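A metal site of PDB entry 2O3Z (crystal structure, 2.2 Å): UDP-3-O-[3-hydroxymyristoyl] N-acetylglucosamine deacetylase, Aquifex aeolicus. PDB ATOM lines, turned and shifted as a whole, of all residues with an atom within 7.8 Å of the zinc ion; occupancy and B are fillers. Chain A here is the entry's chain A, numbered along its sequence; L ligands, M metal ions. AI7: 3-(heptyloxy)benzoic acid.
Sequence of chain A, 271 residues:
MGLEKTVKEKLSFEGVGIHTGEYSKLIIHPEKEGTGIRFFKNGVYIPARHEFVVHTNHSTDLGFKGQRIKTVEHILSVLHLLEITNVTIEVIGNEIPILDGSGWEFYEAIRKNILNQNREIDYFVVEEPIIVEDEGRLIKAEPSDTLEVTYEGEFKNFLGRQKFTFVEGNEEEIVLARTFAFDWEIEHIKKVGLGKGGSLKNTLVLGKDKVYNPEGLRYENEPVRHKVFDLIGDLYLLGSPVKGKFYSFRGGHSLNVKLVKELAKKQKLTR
ND1 of His 226 lies within hydrogen-bond range of O of Arg 178. O of Ala 177 is in hydrogen-bond range of ND1 of His 226 (2.9 Å).
The zinc ion is bound by a ring nitrogen (NE2) of His 226 (2.1 Å), a ring nitrogen (NE2) of His 74 (2.1 Å) and the side-chain carboxylate (OD1) of Asp 230 (2.1 Å). Slightly farther from the zinc ion lies OD2 of Asp 230 (2.6 Å).
Three residues have an atom within 4 Å of the zinc ion: His 74, His 226 and Asp 230. The nearest printed residue that does not touch the zinc ion is Glu 73 (4.2 Å).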
ATOM      1  N   HIS A  58      -1.602   7.374   6.969  1.00  0.00           N
ATOM      2  CA  HIS A  58      -0.644   8.491   6.883  1.00  0.00           C
ATOM      3  C   HIS A  58      -1.251   9.883   6.708  1.00  0.00           C
ATOM      4  O   HIS A  58      -0.532  10.881   6.674  1.00  0.00           O
ATOM      5  CB  HIS A  58       0.385   8.202   5.795  1.00  0.00           C
ATOM      6  CG  HIS A  58       1.102   6.905   5.986  1.00  0.00           C
ATOM      7  ND1 HIS A  58       1.866   6.646   7.103  1.00  0.00           N
ATOM      8  CD2 HIS A  58       1.114   5.767   5.248  1.00  0.00           C
ATOM      9  CE1 HIS A  58       2.318   5.412   7.043  1.00  0.00           C
ATOM     10  NE2 HIS A  58       1.869   4.851   5.929  1.00  0.00           N
ATOM     11  N   SER A  59      -2.575   9.931   6.584  1.00  0.00           N
ATOM     12  CA  SER A  59      -3.306  11.195   6.471  1.00  0.00           C
ATOM     13  C   SER A  59      -4.793  10.907   6.379  1.00  0.00           C
ATOM     14  O   SER A  59      -5.202   9.754   6.191  1.00  0.00           O
ATOM     15  CB  SER A  59      -2.835  12.028   5.257  1.00  0.00           C
ATOM     16  OG  SER A  59      -3.131  11.431   4.009  1.00  0.00           O
ATOM     17  N   THR A  71      -4.978  15.010   3.225  1.00  0.00           N
ATOM     18  CA  THR A  71      -4.478  15.657   4.425  1.00  0.00           C
ATOM     19  C   THR A  71      -5.290  16.842   4.943  1.00  0.00           C
ATOM     20  O   THR A  71      -4.799  17.957   5.007  1.00  0.00           O
ATOM     21  CB  THR A  71      -3.021  16.086   4.168  1.00  0.00           C
ATOM     22  OG1 THR A  71      -2.401  15.056   3.381  1.00  0.00           O
ATOM     23  CG2 THR A  71      -2.229  16.262   5.474  1.00  0.00           C
ATOM     24  N   GLU A  73      -6.686  16.828   8.060  1.00  0.00           N
ATOM     25  CA  GLU A  73      -6.721  16.805   9.521  1.00  0.00           C
ATOM     26  C   GLU A  73      -6.245  18.064  10.252  1.00  0.00           C
ATOM     27  O   GLU A  73      -6.842  18.445  11.255  1.00  0.00           O
ATOM     28  CB  GLU A  73      -5.977  15.582  10.063  1.00  0.00           C
ATOM     29  CG  GLU A  73      -4.497  15.508   9.683  1.00  0.00           C
ATOM     30  CD  GLU A  73      -4.242  14.657   8.453  1.00  0.00           C
ATOM     31  OE1 GLU A  73      -5.092  14.656   7.552  1.00  0.00           O
ATOM     32  OE2 GLU A  73      -3.169  13.996   8.392  1.00  0.00           O
ATOM     33  N   HIS A  74      -5.194  18.700   9.758  1.00  0.00           N
ATOM     34  CA  HIS A  74      -4.652  19.880  10.423  1.00  0.00           C
ATOM     35  C   HIS A  74      -5.530  21.119  10.308  1.00  0.00           C
ATOM     36  O   HIS A  74      -5.746  21.825  11.293  1.00  0.00           O
ATOM     37  CB  HIS A  74      -3.238  20.174   9.911  1.00  0.00           C
ATOM     38  CG  HIS A  74      -2.283  19.044  10.148  1.00  0.00           C
ATOM     39  ND1 HIS A  74      -1.011  19.011   9.608  1.00  0.00           N
ATOM     40  CD2 HIS A  74      -2.421  17.892  10.860  1.00  0.00           C
ATOM     41  CE1 HIS A  74      -0.421  17.896   9.962  1.00  0.00           C
ATOM     42  NE2 HIS A  74      -1.243  17.196  10.715  1.00  0.00           N
ATOM     43  N   ILE A  98       0.986  21.606   3.737  1.00  0.00           N
ATOM     44  CA  ILE A  98       1.442  21.137   5.043  1.00  0.00           C
ATOM     45  C   ILE A  98       2.111  22.269   5.841  1.00  0.00           C
ATOM     46  O   ILE A  98       2.187  22.202   7.069  1.00  0.00           O
ATOM     47  CB  ILE A  98       2.450  19.967   4.906  1.00  0.00           C
ATOM     48  CG1 ILE A  98       2.784  19.387   6.282  1.00  0.00           C
ATOM     49  CG2 ILE A  98       3.741  20.452   4.240  1.00  0.00           C
ATOM     50  CD1 ILE A  98       1.586  18.777   7.000  1.00  0.00           C
ATOM     51  N   GLY A 101       4.035  21.923   9.152  1.00  0.00           N
ATOM     52  CA  GLY A 101       3.661  20.641   9.734  1.00  0.00           C
ATOM     53  C   GLY A 101       2.769  20.719  10.964  1.00  0.00           C
ATOM     54  O   GLY A 101       2.337  19.684  11.479  1.00  0.00           O
ATOM     55  N   SER A 102       2.491  21.920  11.452  1.00  0.00           N
ATOM     56  CA  SER A 102       1.628  22.087  12.617  1.00  0.00           C
ATOM     57  C   SER A 102       0.413  22.891  12.179  1.00  0.00           C
ATOM     58  O   SER A 102       0.199  23.110  10.985  1.00  0.00           O
ATOM     59  CB  SER A 102       2.370  22.812  13.742  1.00  0.00           C
ATOM     60  OG  SER A 102       2.553  24.189  13.428  1.00  0.00           O
ATOM     61  N   ALA A 177       2.682  21.796  17.769  1.00  0.00           N
ATOM     62  CA  ALA A 177       3.291  20.467  17.625  1.00  0.00           C
ATOM     63  C   ALA A 177       3.351  20.043  16.159  1.00  0.00           C
ATOM     64  O   ALA A 177       2.318  19.894  15.511  1.00  0.00           O
ATOM     65  CB  ALA A 177       2.519  19.440  18.452  1.00  0.00           C
ATOM     66  N   ARG A 178       4.561  19.815  15.654  1.00  0.00           N
ATOM     67  CA  ARG A 178       4.732  19.428  14.262  1.00  0.00           C
ATOM     68  C   ARG A 178       4.491  17.955  13.926  1.00  0.00           C
ATOM     69  O   ARG A 178       4.492  17.091  14.804  1.00  0.00           O
ATOM     70  CB  ARG A 178       6.146  19.779  13.780  1.00  0.00           C
ATOM     71  CG  ARG A 178       6.487  21.258  13.878  1.00  0.00           C
ATOM     72  CD  ARG A 178       7.723  21.442  14.743  1.00  0.00           C
ATOM     73  NE  ARG A 178       8.959  21.118  14.041  1.00  0.00           N
ATOM     74  CZ  ARG A 178      10.105  20.824  14.638  1.00  0.00           C
ATOM     75  NH1 ARG A 178      10.176  20.808  15.972  1.00  0.00           N
ATOM     76  NH2 ARG A 178      11.179  20.587  13.913  1.00  0.00           N
ATOM     77  N   THR A 179       4.294  17.713  12.640  1.00  0.00           N
ATOM     78  CA  THR A 179       4.094  16.374  12.102  1.00  0.00           C
ATOM     79  C   THR A 179       5.395  15.629  12.393  1.00  0.00           C
ATOM     80  O   THR A 179       6.468  16.232  12.394  1.00  0.00           O
ATOM     81  CB  THR A 179       3.924  16.459  10.565  1.00  0.00           C
ATOM     82  OG1 THR A 179       2.675  17.088  10.243  1.00  0.00           O
ATOM     83  CG2 THR A 179       3.999  15.091   9.936  1.00  0.00           C
ATOM     84  N   PHE A 180       5.308  14.328  12.626  1.00  0.00           N
ATOM     85  CA  PHE A 180       6.506  13.553  12.887  1.00  0.00           C
ATOM     86  C   PHE A 180       6.410  12.170  12.244  1.00  0.00           C
ATOM     87  O   PHE A 180       5.329  11.717  11.836  1.00  0.00           O
ATOM     88  CB  PHE A 180       6.742  13.416  14.396  1.00  0.00           C
ATOM     89  CG  PHE A 180       5.815  12.454  15.076  1.00  0.00           C
ATOM     90  CD1 PHE A 180       6.177  11.124  15.247  1.00  0.00           C
ATOM     91  CD2 PHE A 180       4.571  12.874  15.523  1.00  0.00           C
ATOM     92  CE1 PHE A 180       5.312  10.208  15.862  1.00  0.00           C
ATOM     93  CE2 PHE A 180       3.687  11.973  16.139  1.00  0.00           C
ATOM     94  CZ  PHE A 180       4.065  10.636  16.306  1.00  0.00           C
ATOM     95  N   HIS A 226       1.048  16.304  19.005  1.00  0.00           N
ATOM     96  CA  HIS A 226       0.587  16.324  17.629  1.00  0.00           C
ATOM     97  C   HIS A 226      -0.507  15.288  17.408  1.00  0.00           C
ATOM     98  O   HIS A 226      -1.477  15.543  16.677  1.00  0.00           O
ATOM     99  CB  HIS A 226       1.729  16.080  16.636  1.00  0.00           C
ATOM    100  CG  HIS A 226       1.296  16.206  15.213  1.00  0.00           C
ATOM    101  ND1 HIS A 226       1.216  17.424  14.571  1.00  0.00           N
ATOM    102  CD2 HIS A 226       0.809  15.293  14.352  1.00  0.00           C
ATOM    103  CE1 HIS A 226       0.681  17.245  13.379  1.00  0.00           C
ATOM    104  NE2 HIS A 226       0.418  15.965  13.217  1.00  0.00           N
ATOM    105  N   LYS A 227      -0.365  14.120  18.028  1.00  0.00           N
ATOM    106  CA  LYS A 227      -1.376  13.080  17.892  1.00  0.00           C
ATOM    107  C   LYS A 227      -2.725  13.582  18.424  1.00  0.00           C
ATOM    108  O   LYS A 227      -3.779  13.243  17.868  1.00  0.00           O
ATOM    109  CB  LYS A 227      -0.941  11.827  18.647  1.00  0.00           C
ATOM    110  CG  LYS A 227       0.091  10.983  17.898  1.00  0.00           C
ATOM    111  CD  LYS A 227      -0.540  10.299  16.704  1.00  0.00           C
ATOM    112  CE  LYS A 227       0.358   9.227  16.124  1.00  0.00           C
ATOM    113  NZ  LYS A 227      -0.408   8.330  15.204  1.00  0.00           N
ATOM    114  N   PHE A 229      -3.637  16.700  18.408  1.00  0.00           N
ATOM    115  CA  PHE A 229      -4.028  17.672  17.376  1.00  0.00           C
ATOM    116  C   PHE A 229      -4.714  16.951  16.203  1.00  0.00           C
ATOM    117  O   PHE A 229      -5.758  17.398  15.726  1.00  0.00           O
ATOM    118  CB  PHE A 229      -2.768  18.416  16.887  1.00  0.00           C
ATOM    119  CG  PHE A 229      -3.025  19.430  15.828  1.00  0.00           C
ATOM    120  CD1 PHE A 229      -3.727  20.602  16.106  1.00  0.00           C
ATOM    121  CD2 PHE A 229      -2.548  19.233  14.533  1.00  0.00           C
ATOM    122  CE1 PHE A 229      -3.952  21.564  15.114  1.00  0.00           C
ATOM    123  CE2 PHE A 229      -2.763  20.182  13.525  1.00  0.00           C
ATOM    124  CZ  PHE A 229      -3.472  21.358  13.822  1.00  0.00           C
ATOM    125  N   ASP A 230      -4.133  15.843  15.736  1.00  0.00           N
ATOM    126  CA  ASP A 230      -4.713  15.076  14.634  1.00  0.00           C
ATOM    127  C   ASP A 230      -6.089  14.523  14.993  1.00  0.00           C
ATOM    128  O   ASP A 230      -7.017  14.586  14.191  1.00  0.00           O
ATOM    129  CB  ASP A 230      -3.823  13.872  14.257  1.00  0.00           C
ATOM    130  CG  ASP A 230      -2.653  14.247  13.367  1.00  0.00           C
ATOM    131  OD1 ASP A 230      -2.655  15.346  12.780  1.00  0.00           O
ATOM    132  OD2 ASP A 230      -1.737  13.430  13.233  1.00  0.00           O
ATOM    133  N   LEU A 231      -6.228  13.974  16.193  1.00  0.00           N
ATOM    134  CA  LEU A 231      -7.487  13.395  16.632  1.00  0.00           C
ATOM    135  C   LEU A 231      -8.598  14.440  16.696  1.00  0.00           C
ATOM    136  O   LEU A 231      -9.747  14.173  16.339  1.00  0.00           O
ATOM    137  CB  LEU A 231      -7.289  12.731  17.990  1.00  0.00           C
ATOM    138  CG  LEU A 231      -8.517  12.173  18.728  1.00  0.00           C
ATOM    139  CD1 LEU A 231      -9.395  11.366  17.769  1.00  0.00           C
ATOM    140  CD2 LEU A 231      -8.034  11.297  19.890  1.00  0.00           C
ATOM    141  N   HIS A 253      -5.164   7.863  12.446  1.00  0.00           N
ATOM    142  CA  HIS A 253      -6.327   8.302  11.679  1.00  0.00           C
ATOM    143  C   HIS A 253      -7.366   7.197  11.461  1.00  0.00           C
ATOM    144  O   HIS A 253      -8.556   7.433  11.634  1.00  0.00           O
ATOM    145  CB  HIS A 253      -5.893   8.854  10.333  1.00  0.00           C
ATOM    146  CG  HIS A 253      -5.047  10.081  10.442  1.00  0.00           C
ATOM    147  ND1 HIS A 253      -5.502  11.248  11.027  1.00  0.00           N
ATOM    148  CD2 HIS A 253      -3.765  10.319  10.070  1.00  0.00           C
ATOM    149  CE1 HIS A 253      -4.527  12.152  11.019  1.00  0.00           C
ATOM    150  NE2 HIS A 253      -3.466  11.610  10.438  1.00  0.00           N
HETATM  151  C1  AI7 L   1      11.426  13.168   3.421  1.00  0.00           C
HETATM  152  C2  AI7 L   1      12.885  14.178   5.616  1.00  0.00           C
HETATM  153  C3  AI7 L   1      13.437  14.279   4.309  1.00  0.00           C
HETATM  154  C4  AI7 L   1       4.645  11.986   7.267  1.00  0.00           C
HETATM  155  C5  AI7 L   1      13.276  13.867   1.805  1.00  0.00           C
HETATM  156  C6  AI7 L   1       7.589  11.633   5.766  1.00  0.00           C
HETATM  157  C7  AI7 L   1      11.608  13.576   5.803  1.00  0.00           C
HETATM  158  C8  AI7 L   1       8.851  12.461   5.987  1.00  0.00           C
HETATM  159  C9  AI7 L   1       2.915  11.435   9.032  1.00  0.00           C
HETATM  160  C10 AI7 L   1       3.304  11.303   7.548  1.00  0.00           C
HETATM  161  C11 AI7 L   1      10.836  13.059   4.716  1.00  0.00           C
HETATM  162  C12 AI7 L   1       5.042  11.858   5.785  1.00  0.00           C
HETATM  163  C13 AI7 L   1       6.383  12.547   5.491  1.00  0.00           C
HETATM  164  C14 AI7 L   1      12.705  13.766   3.191  1.00  0.00           C
HETATM  165  O15 AI7 L   1      14.463  14.431   1.551  1.00  0.00           O
HETATM  166  O16 AI7 L   1       9.591  12.448   4.786  1.00  0.00           O
HETATM  167  O17 AI7 L   1      12.661  13.441   0.828  1.00  0.00           O
HETATM  168 ZN    ZN M   1      -0.852  15.399  11.703  1.00  0.00          ZN
